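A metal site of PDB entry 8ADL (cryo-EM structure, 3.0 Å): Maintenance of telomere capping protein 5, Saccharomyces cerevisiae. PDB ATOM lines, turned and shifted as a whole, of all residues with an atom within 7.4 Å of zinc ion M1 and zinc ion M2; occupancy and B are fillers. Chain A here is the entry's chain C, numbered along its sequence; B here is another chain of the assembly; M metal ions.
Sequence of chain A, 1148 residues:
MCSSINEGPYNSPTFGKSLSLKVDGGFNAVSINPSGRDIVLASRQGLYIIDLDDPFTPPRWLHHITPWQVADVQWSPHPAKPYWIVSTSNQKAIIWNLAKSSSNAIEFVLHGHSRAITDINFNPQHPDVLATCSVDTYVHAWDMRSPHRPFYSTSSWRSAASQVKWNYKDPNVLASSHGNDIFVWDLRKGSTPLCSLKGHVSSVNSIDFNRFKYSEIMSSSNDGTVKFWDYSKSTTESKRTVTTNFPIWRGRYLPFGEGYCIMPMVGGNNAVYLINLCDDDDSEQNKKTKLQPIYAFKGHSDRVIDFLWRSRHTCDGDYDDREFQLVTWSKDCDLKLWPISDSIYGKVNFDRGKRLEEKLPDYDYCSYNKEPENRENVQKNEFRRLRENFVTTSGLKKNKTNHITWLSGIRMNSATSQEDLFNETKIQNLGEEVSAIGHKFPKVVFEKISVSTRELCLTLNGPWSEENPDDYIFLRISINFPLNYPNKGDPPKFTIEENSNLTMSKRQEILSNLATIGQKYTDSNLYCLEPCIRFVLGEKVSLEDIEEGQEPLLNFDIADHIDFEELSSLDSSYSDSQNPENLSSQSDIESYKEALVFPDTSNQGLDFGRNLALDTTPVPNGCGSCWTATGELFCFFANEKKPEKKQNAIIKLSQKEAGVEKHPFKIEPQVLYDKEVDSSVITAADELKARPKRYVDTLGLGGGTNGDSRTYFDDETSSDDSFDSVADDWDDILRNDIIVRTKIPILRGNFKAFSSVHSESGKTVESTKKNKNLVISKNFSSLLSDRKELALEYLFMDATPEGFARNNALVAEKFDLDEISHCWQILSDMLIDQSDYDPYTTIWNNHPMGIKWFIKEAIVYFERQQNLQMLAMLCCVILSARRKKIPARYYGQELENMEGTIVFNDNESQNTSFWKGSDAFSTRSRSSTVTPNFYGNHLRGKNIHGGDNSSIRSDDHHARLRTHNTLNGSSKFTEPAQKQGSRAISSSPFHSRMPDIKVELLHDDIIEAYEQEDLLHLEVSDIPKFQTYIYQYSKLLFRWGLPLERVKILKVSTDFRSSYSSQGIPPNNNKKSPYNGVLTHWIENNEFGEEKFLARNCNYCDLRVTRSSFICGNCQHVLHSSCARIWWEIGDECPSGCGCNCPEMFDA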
ATOM      1  N   ASN A1099       3.946 -25.198   0.586  1.00  0.00           N
ATOM      2  CA  ASN A1099       4.765 -24.552  -0.427  1.00  0.00           C
ATOM      3  C   ASN A1099       5.254 -25.505  -1.510  1.00  0.00           C
ATOM      4  O   ASN A1099       5.996 -25.090  -2.400  1.00  0.00           O
ATOM      5  CB  ASN A1099       5.965 -23.869   0.235  1.00  0.00           C
ATOM      6  CG  ASN A1099       5.557 -22.647   1.034  1.00  0.00           C
ATOM      7  OD1 ASN A1099       5.387 -21.562   0.477  1.00  0.00           O
ATOM      8  ND2 ASN A1099       5.387 -22.825   2.337  1.00  0.00           N
ATOM      9  N   PHE A1110       6.129 -29.359   8.466  1.00  0.00           N
ATOM     10  CA  PHE A1110       7.539 -29.069   8.649  1.00  0.00           C
ATOM     11  C   PHE A1110       7.742 -27.554   8.587  1.00  0.00           C
ATOM     12  O   PHE A1110       7.304 -26.910   7.635  1.00  0.00           O
ATOM     13  CB  PHE A1110       8.388 -29.759   7.573  1.00  0.00           C
ATOM     14  CG  PHE A1110       9.735 -29.132   7.350  1.00  0.00           C
ATOM     15  CD1 PHE A1110      10.722 -29.186   8.324  1.00  0.00           C
ATOM     16  CD2 PHE A1110      10.020 -28.491   6.155  1.00  0.00           C
ATOM     17  CE1 PHE A1110      11.963 -28.605   8.115  1.00  0.00           C
ATOM     18  CE2 PHE A1110      11.256 -27.915   5.940  1.00  0.00           C
ATOM     19  CZ  PHE A1110      12.230 -27.975   6.928  1.00  0.00           C
ATOM     20  N   ILE A1111       8.391 -27.001   9.608  1.00  0.00           N
ATOM     21  CA  ILE A1111       8.585 -25.564   9.727  1.00  0.00           C
ATOM     22  C   ILE A1111      10.072 -25.267   9.756  1.00  0.00           C
ATOM     23  O   ILE A1111      10.819 -25.856  10.553  1.00  0.00           O
ATOM     24  CB  ILE A1111       7.893 -25.006  10.989  1.00  0.00           C
ATOM     25  CG1 ILE A1111       6.429 -25.446  11.042  1.00  0.00           C
ATOM     26  CG2 ILE A1111       8.004 -23.491  11.030  1.00  0.00           C
ATOM     27  CD1 ILE A1111       5.819 -25.366  12.414  1.00  0.00           C
ATOM     28  N   CYS A1112      10.511 -24.347   8.899  1.00  0.00           N
ATOM     29  CA  CYS A1112      11.839 -23.780   8.939  1.00  0.00           C
ATOM     30  C   CYS A1112      11.875 -22.564   9.852  1.00  0.00           C
ATOM     31  O   CYS A1112      10.851 -21.920  10.120  1.00  0.00           O
ATOM     32  CB  CYS A1112      12.299 -23.392   7.533  1.00  0.00           C
ATOM     33  SG  CYS A1112      13.957 -22.674   7.464  1.00  0.00           S
ATOM     34  N   GLY A1113      13.069 -22.242  10.335  1.00  0.00           N
ATOM     35  CA  GLY A1113      13.220 -21.130  11.259  1.00  0.00           C
ATOM     36  C   GLY A1113      13.647 -19.832  10.600  1.00  0.00           C
ATOM     37  O   GLY A1113      13.137 -18.759  10.955  1.00  0.00           O
ATOM     38  N   ASN A1114      14.583 -19.905   9.648  1.00  0.00           N
ATOM     39  CA  ASN A1114      15.040 -18.715   8.953  1.00  0.00           C
ATOM     40  C   ASN A1114      13.933 -18.129   8.082  1.00  0.00           C
ATOM     41  O   ASN A1114      13.635 -16.929   8.148  1.00  0.00           O
ATOM     42  CB  ASN A1114      16.280 -19.026   8.115  1.00  0.00           C
ATOM     43  CG  ASN A1114      17.111 -17.799   7.826  1.00  0.00           C
ATOM     44  OD1 ASN A1114      16.810 -16.700   8.288  1.00  0.00           O
ATOM     45  ND2 ASN A1114      18.176 -17.976   7.049  1.00  0.00           N
ATOM     46  N   CYS A1115      13.318 -18.961   7.246  1.00  0.00           N
ATOM     47  CA  CYS A1115      12.108 -18.595   6.524  1.00  0.00           C
ATOM     48  C   CYS A1115      10.913 -19.284   7.182  1.00  0.00           C
ATOM     49  O   CYS A1115      11.007 -20.439   7.615  1.00  0.00           O
ATOM     50  CB  CYS A1115      12.207 -18.971   5.041  1.00  0.00           C
ATOM     51  SG  CYS A1115      12.018 -20.717   4.638  1.00  0.00           S
ATOM     52  N   GLN A1116       9.811 -18.559   7.293  1.00  0.00           N
ATOM     53  CA  GLN A1116       8.654 -19.050   8.030  1.00  0.00           C
ATOM     54  C   GLN A1116       7.626 -19.624   7.064  1.00  0.00           C
ATOM     55  O   GLN A1116       6.563 -19.062   6.805  1.00  0.00           O
ATOM     56  CB  GLN A1116       8.073 -17.937   8.897  1.00  0.00           C
ATOM     57  CG  GLN A1116       9.004 -17.539  10.036  1.00  0.00           C
ATOM     58  CD  GLN A1116       8.615 -16.226  10.697  1.00  0.00           C
ATOM     59  OE1 GLN A1116       7.509 -15.712  10.476  1.00  0.00           O
ATOM     60  NE2 GLN A1116       9.512 -15.671  11.487  1.00  0.00           N
ATOM     61  N   HIS A1117       7.971 -20.791   6.513  1.00  0.00           N
ATOM     62  CA  HIS A1117       7.188 -21.450   5.483  1.00  0.00           C
ATOM     63  C   HIS A1117       6.876 -22.890   5.887  1.00  0.00           C
ATOM     64  O   HIS A1117       7.746 -23.597   6.390  1.00  0.00           O
ATOM     65  CB  HIS A1117       7.908 -21.438   4.134  1.00  0.00           C
ATOM     66  CG  HIS A1117       8.044 -20.076   3.531  1.00  0.00           C
ATOM     67  ND1 HIS A1117       9.148 -19.694   2.798  1.00  0.00           N
ATOM     68  CD2 HIS A1117       7.221 -19.000   3.550  1.00  0.00           C
ATOM     69  CE1 HIS A1117       9.000 -18.447   2.402  1.00  0.00           C
ATOM     70  NE2 HIS A1117       7.833 -18.000   2.835  1.00  0.00           N
ATOM     71  N   VAL A1118       5.629 -23.309   5.648  1.00  0.00           N
ATOM     72  CA  VAL A1118       5.182 -24.655   5.992  1.00  0.00           C
ATOM     73  C   VAL A1118       5.472 -25.609   4.835  1.00  0.00           C
ATOM     74  O   VAL A1118       5.632 -25.196   3.682  1.00  0.00           O
ATOM     75  CB  VAL A1118       3.691 -24.677   6.344  1.00  0.00           C
ATOM     76  CG1 VAL A1118       3.438 -23.959   7.637  1.00  0.00           C
ATOM     77  CG2 VAL A1118       2.879 -24.059   5.227  1.00  0.00           C
ATOM     78  N   TRP A1128      13.102 -32.742  -0.253  1.00  0.00           N
ATOM     79  CA  TRP A1128      14.491 -32.683   0.199  1.00  0.00           C
ATOM     80  C   TRP A1128      15.317 -33.860  -0.265  1.00  0.00           C
ATOM     81  O   TRP A1128      16.530 -33.880  -0.026  1.00  0.00           O
ATOM     82  CB  TRP A1128      14.562 -32.551   1.719  1.00  0.00           C
ATOM     83  CG  TRP A1128      13.859 -31.336   2.277  1.00  0.00           C
ATOM     84  CD1 TRP A1128      12.914 -31.325   3.263  1.00  0.00           C
ATOM     85  CD2 TRP A1128      14.059 -29.970   1.897  1.00  0.00           C
ATOM     86  NE1 TRP A1128      12.505 -30.041   3.506  1.00  0.00           N
ATOM     87  CE2 TRP A1128      13.190 -29.189   2.690  1.00  0.00           C
ATOM     88  CE3 TRP A1128      14.880 -29.322   0.970  1.00  0.00           C
ATOM     89  CZ2 TRP A1128      13.123 -27.808   2.575  1.00  0.00           C
ATOM     90  CZ3 TRP A1128      14.807 -27.957   0.855  1.00  0.00           C
ATOM     91  CH2 TRP A1128      13.938 -27.214   1.646  1.00  0.00           C
ATOM     92  N   GLU A1133      16.868 -25.684  -1.779  1.00  0.00           N
ATOM     93  CA  GLU A1133      16.339 -24.436  -1.239  1.00  0.00           C
ATOM     94  C   GLU A1133      14.855 -24.596  -0.942  1.00  0.00           C
ATOM     95  O   GLU A1133      14.261 -25.656  -1.195  1.00  0.00           O
ATOM     96  CB  GLU A1133      16.566 -23.275  -2.213  1.00  0.00           C
ATOM     97  CG  GLU A1133      18.034 -22.978  -2.491  1.00  0.00           C
ATOM     98  CD  GLU A1133      18.212 -21.779  -3.393  1.00  0.00           C
ATOM     99  OE1 GLU A1133      17.202 -21.255  -3.902  1.00  0.00           O
ATOM    100  OE2 GLU A1133      19.376 -21.346  -3.580  1.00  0.00           O
ATOM    101  N   CYS A1134      14.255 -23.546  -0.410  1.00  0.00           N
ATOM    102  CA  CYS A1134      12.824 -23.558  -0.114  1.00  0.00           C
ATOM    103  C   CYS A1134      12.026 -23.632  -1.412  1.00  0.00           C
ATOM    104  O   CYS A1134      12.358 -22.936  -2.376  1.00  0.00           O
ATOM    105  CB  CYS A1134      12.445 -22.316   0.691  1.00  0.00           C
ATOM    106  SG  CYS A1134      10.754 -22.296   1.335  1.00  0.00           S
ATOM    107  N   PRO A1135      10.992 -24.478  -1.476  1.00  0.00           N
ATOM    108  CA  PRO A1135      10.213 -24.590  -2.719  1.00  0.00           C
ATOM    109  C   PRO A1135       9.417 -23.345  -3.075  1.00  0.00           C
ATOM    110  O   PRO A1135       8.984 -23.230  -4.229  1.00  0.00           O
ATOM    111  CB  PRO A1135       9.280 -25.779  -2.432  1.00  0.00           C
ATOM    112  CG  PRO A1135       9.218 -25.869  -0.956  1.00  0.00           C
ATOM    113  CD  PRO A1135      10.556 -25.445  -0.457  1.00  0.00           C
ATOM    114  N   SER A1136       9.213 -22.415  -2.147  1.00  0.00           N
ATOM    115  CA  SER A1136       8.606 -21.133  -2.476  1.00  0.00           C
ATOM    116  C   SER A1136       9.585 -20.177  -3.133  1.00  0.00           C
ATOM    117  O   SER A1136       9.172 -19.094  -3.566  1.00  0.00           O
ATOM    118  CB  SER A1136       8.019 -20.492  -1.226  1.00  0.00           C
ATOM    119  OG  SER A1136       8.963 -20.430  -0.183  1.00  0.00           O
ATOM    120  N   GLY A1137      10.868 -20.539  -3.207  1.00  0.00           N
ATOM    121  CA  GLY A1137      11.873 -19.721  -3.847  1.00  0.00           C
ATOM    122  C   GLY A1137      12.197 -18.432  -3.113  1.00  0.00           C
ATOM    123  O   GLY A1137      12.361 -17.388  -3.763  1.00  0.00           O
ATOM    124  N   CYS A1138      12.300 -18.481  -1.798  1.00  0.00           N
ATOM    125  CA  CYS A1138      12.735 -17.328  -1.015  1.00  0.00           C
ATOM    126  C   CYS A1138      14.242 -17.254  -0.844  1.00  0.00           C
ATOM    127  O   CYS A1138      14.744 -16.283  -0.279  1.00  0.00           O
ATOM    128  CB  CYS A1138      12.055 -17.333   0.357  1.00  0.00           C
ATOM    129  SG  CYS A1138      12.356 -18.827   1.332  1.00  0.00           S
ATOM    130  N   GLY A1139      14.978 -18.263  -1.325  1.00  0.00           N
ATOM    131  CA  GLY A1139      16.418 -18.243  -1.208  1.00  0.00           C
ATOM    132  C   GLY A1139      16.966 -18.743   0.110  1.00  0.00           C
ATOM    133  O   GLY A1139      18.133 -18.479   0.420  1.00  0.00           O
ATOM    134  N   CYS A1140      16.175 -19.453   0.897  1.00  0.00           N
ATOM    135  CA  CYS A1140      16.579 -19.943   2.207  1.00  0.00           C
ATOM    136  C   CYS A1140      17.015 -21.398   2.093  1.00  0.00           C
ATOM    137  O   CYS A1140      16.230 -22.249   1.671  1.00  0.00           O
ATOM    138  CB  CYS A1140      15.450 -19.799   3.220  1.00  0.00           C
ATOM    139  SG  CYS A1140      15.803 -20.588   4.812  1.00  0.00           S
ATOM    140  N   ASN A1141      18.259 -21.681   2.478  1.00  0.00           N
ATOM    141  CA  ASN A1141      18.782 -23.043   2.507  1.00  0.00           C
ATOM    142  C   ASN A1141      18.256 -23.730   3.767  1.00  0.00           C
ATOM    143  O   ASN A1141      18.915 -23.792   4.804  1.00  0.00           O
ATOM    144  CB  ASN A1141      20.305 -23.040   2.451  1.00  0.00           C
ATOM    145  CG  ASN A1141      20.847 -22.105   1.384  1.00  0.00           C
ATOM    146  OD1 ASN A1141      20.660 -22.340   0.191  1.00  0.00           O
ATOM    147  ND2 ASN A1141      21.524 -21.045   1.819  1.00  0.00           N
ATOM    148  N   CYS A1142      17.031 -24.238   3.647  1.00  0.00           N
ATOM    149  CA  CYS A1142      16.345 -24.848   4.776  1.00  0.00           C
ATOM    150  C   CYS A1142      17.007 -26.085   5.395  1.00  0.00           C
ATOM    151  O   CYS A1142      16.819 -26.277   6.606  1.00  0.00           O
ATOM    152  CB  CYS A1142      14.905 -25.207   4.357  1.00  0.00           C
ATOM    153  SG  CYS A1142      13.850 -23.809   3.999  1.00  0.00           S
ATOM    154  N   PRO A1143      17.757 -26.937   4.676  1.00  0.00           N
ATOM    155  CA  PRO A1143      18.538 -27.968   5.391  1.00  0.00           C
ATOM    156  C   PRO A1143      19.619 -27.435   6.328  1.00  0.00           C
ATOM    157  O   PRO A1143      20.059 -28.186   7.208  1.00  0.00           O
ATOM    158  CB  PRO A1143      19.158 -28.777   4.247  1.00  0.00           C
ATOM    159  CG  PRO A1143      18.141 -28.731   3.202  1.00  0.00           C
ATOM    160  CD  PRO A1143      17.586 -27.330   3.260  1.00  0.00           C
ATOM    161  N   MET A1145      19.333 -24.048   7.769  1.00  0.00           N
ATOM    162  CA  MET A1145      18.871 -22.864   8.478  1.00  0.00           C
ATOM    163  C   MET A1145      17.486 -23.067   9.091  1.00  0.00           C
ATOM    164  O   MET A1145      16.763 -22.089   9.304  1.00  0.00           O
ATOM    165  CB  MET A1145      18.848 -21.649   7.549  1.00  0.00           C
ATOM    166  CG  MET A1145      20.194 -20.968   7.363  1.00  0.00           C
ATOM    167  SD  MET A1145      20.639 -19.913   8.750  1.00  0.00           S
ATOM    168  CE  MET A1145      22.215 -20.626   9.230  1.00  0.00           C
ATOM    169  N   PHE A1146      17.101 -24.305   9.382  1.00  0.00           N
ATOM    170  CA  PHE A1146      15.802 -24.558   9.991  1.00  0.00           C
ATOM    171  C   PHE A1146      15.826 -24.483  11.515  1.00  0.00           C
ATOM    172  O   PHE A1146      14.793 -24.735  12.144  1.00  0.00           O
ATOM    173  CB  PHE A1146      15.239 -25.909   9.538  1.00  0.00           C
ATOM    174  CG  PHE A1146      15.962 -27.102  10.091  1.00  0.00           C
ATOM    175  CD1 PHE A1146      17.136 -27.553   9.523  1.00  0.00           C
ATOM    176  CD2 PHE A1146      15.434 -27.807  11.161  1.00  0.00           C
ATOM    177  CE1 PHE A1146      17.794 -28.664  10.028  1.00  0.00           C
ATOM    178  CE2 PHE A1146      16.091 -28.916  11.679  1.00  0.00           C
ATOM    179  CZ  PHE A1146      17.265 -29.343  11.108  1.00  0.00           C
ATOM    180  N   ILE B 872       8.010 -13.364  -3.440  1.00  0.00           N
ATOM    181  CA  ILE B 872       7.986 -14.566  -2.616  1.00  0.00           C
ATOM    182  C   ILE B 872       6.762 -14.539  -1.708  1.00  0.00           C
ATOM    183  O   ILE B 872       6.142 -13.497  -1.462  1.00  0.00           O
ATOM    184  CB  ILE B 872       9.273 -14.703  -1.782  1.00  0.00           C
ATOM    185  CG1 ILE B 872       9.410 -13.541  -0.793  1.00  0.00           C
ATOM    186  CG2 ILE B 872      10.486 -14.763  -2.701  1.00  0.00           C
ATOM    187  CD1 ILE B 872      10.502 -13.723   0.229  1.00  0.00           C
ATOM    188  N   LYS B 873       6.414 -15.721  -1.208  1.00  0.00           N
ATOM    189  CA  LYS B 873       5.286 -15.858  -0.291  1.00  0.00           C
ATOM    190  C   LYS B 873       5.636 -15.242   1.057  1.00  0.00           C
ATOM    191  O   LYS B 873       6.761 -15.408   1.544  1.00  0.00           O
ATOM    192  CB  LYS B 873       4.899 -17.326  -0.130  1.00  0.00           C
ATOM    193  CG  LYS B 873       3.562 -17.558   0.553  1.00  0.00           C
ATOM    194  CD  LYS B 873       3.246 -19.029   0.690  1.00  0.00           C
ATOM    195  CE  LYS B 873       2.515 -19.559  -0.531  1.00  0.00           C
ATOM    196  NZ  LYS B 873       1.065 -19.206  -0.492  1.00  0.00           N
ATOM    197  N   GLN B 876       4.517 -17.359   7.162  1.00  0.00           N
ATOM    198  CA  GLN B 876       3.257 -18.047   7.474  1.00  0.00           C
ATOM    199  C   GLN B 876       3.112 -18.403   8.942  1.00  0.00           C
ATOM    200  O   GLN B 876       2.148 -17.980   9.580  1.00  0.00           O
ATOM    201  CB  GLN B 876       3.142 -19.309   6.612  1.00  0.00           C
ATOM    202  CG  GLN B 876       3.230 -19.058   5.119  1.00  0.00           C
ATOM    203  CD  GLN B 876       3.165 -20.340   4.304  1.00  0.00           C
ATOM    204  OE1 GLN B 876       4.125 -21.106   4.248  1.00  0.00           O
ATOM    205  NE2 GLN B 876       2.026 -20.561   3.662  1.00  0.00           N
HETATM  206 ZN    ZN M   1      13.934 -21.881   5.281  1.00  0.00          ZN
HETATM  207 ZN    ZN M   2      11.096 -20.347   2.540  1.00  0.00          ZN
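The side-chain hydroxyl of Ser 1136 sits close to a ring nitrogen (ND1) of His 1117 (3.1 Å). NE2 of His 1117 sits at hydrogen-bond distance from O of Lys 873 of chain B (3.1 Å). The backbone NH (N) of Cys 1134 sits at hydrogen-bond distance from the backbone carbonyl oxygen (O) of Cys 1140 (3.1 Å). The side-chain hydroxyl (OG) of Ser 1136 lies close to the side-chain sulfur (SG) of Cys 1134 (3.0 Å). The side-chain sulfur (SG) of Cys 1112 sits close to the backbone NH (N) of Asn 1114 (3.6 Å). The side-chain sulfur (SG) of Cys 1112 sits close to the backbone carbonyl oxygen (O) of Met 1145 (3.4 Å).
Of the 27 residues printed, 4 come within 4 Å of zinc ion M1.
Merely in contact with zinc ion M2: Ser 1136 (3.5 Å). Along chain A the residues within 4 Å of zinc ion M2 span positions 1115 to 1138. The nearest printed residue that does not touch zinc ion M2 is Cys 1140 (4.4 Å).
SG of Cys 1142 binds zinc ion M1 (2.3 Å). Zinc ion M1 is bound by the side-chain sulfur (SG) of Cys 1140 (2.3 Å). Zinc ion M1 is bound by the side-chain sulfur (SG) of Cys 1112 (2.3 Å). SG of Cys 1115 binds zinc ion M1, 2.3 Å away.
Zinc ion M2 is bound by a ring nitrogen (ND1) of His 1117 (2.1 Å), the side-chain sulfur of Cys 1138 (2.3 Å), the side-chain sulfur of Cys 1134 (2.3 Å) and the side-chain sulfur of Cys 1115 (2.3 Å).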
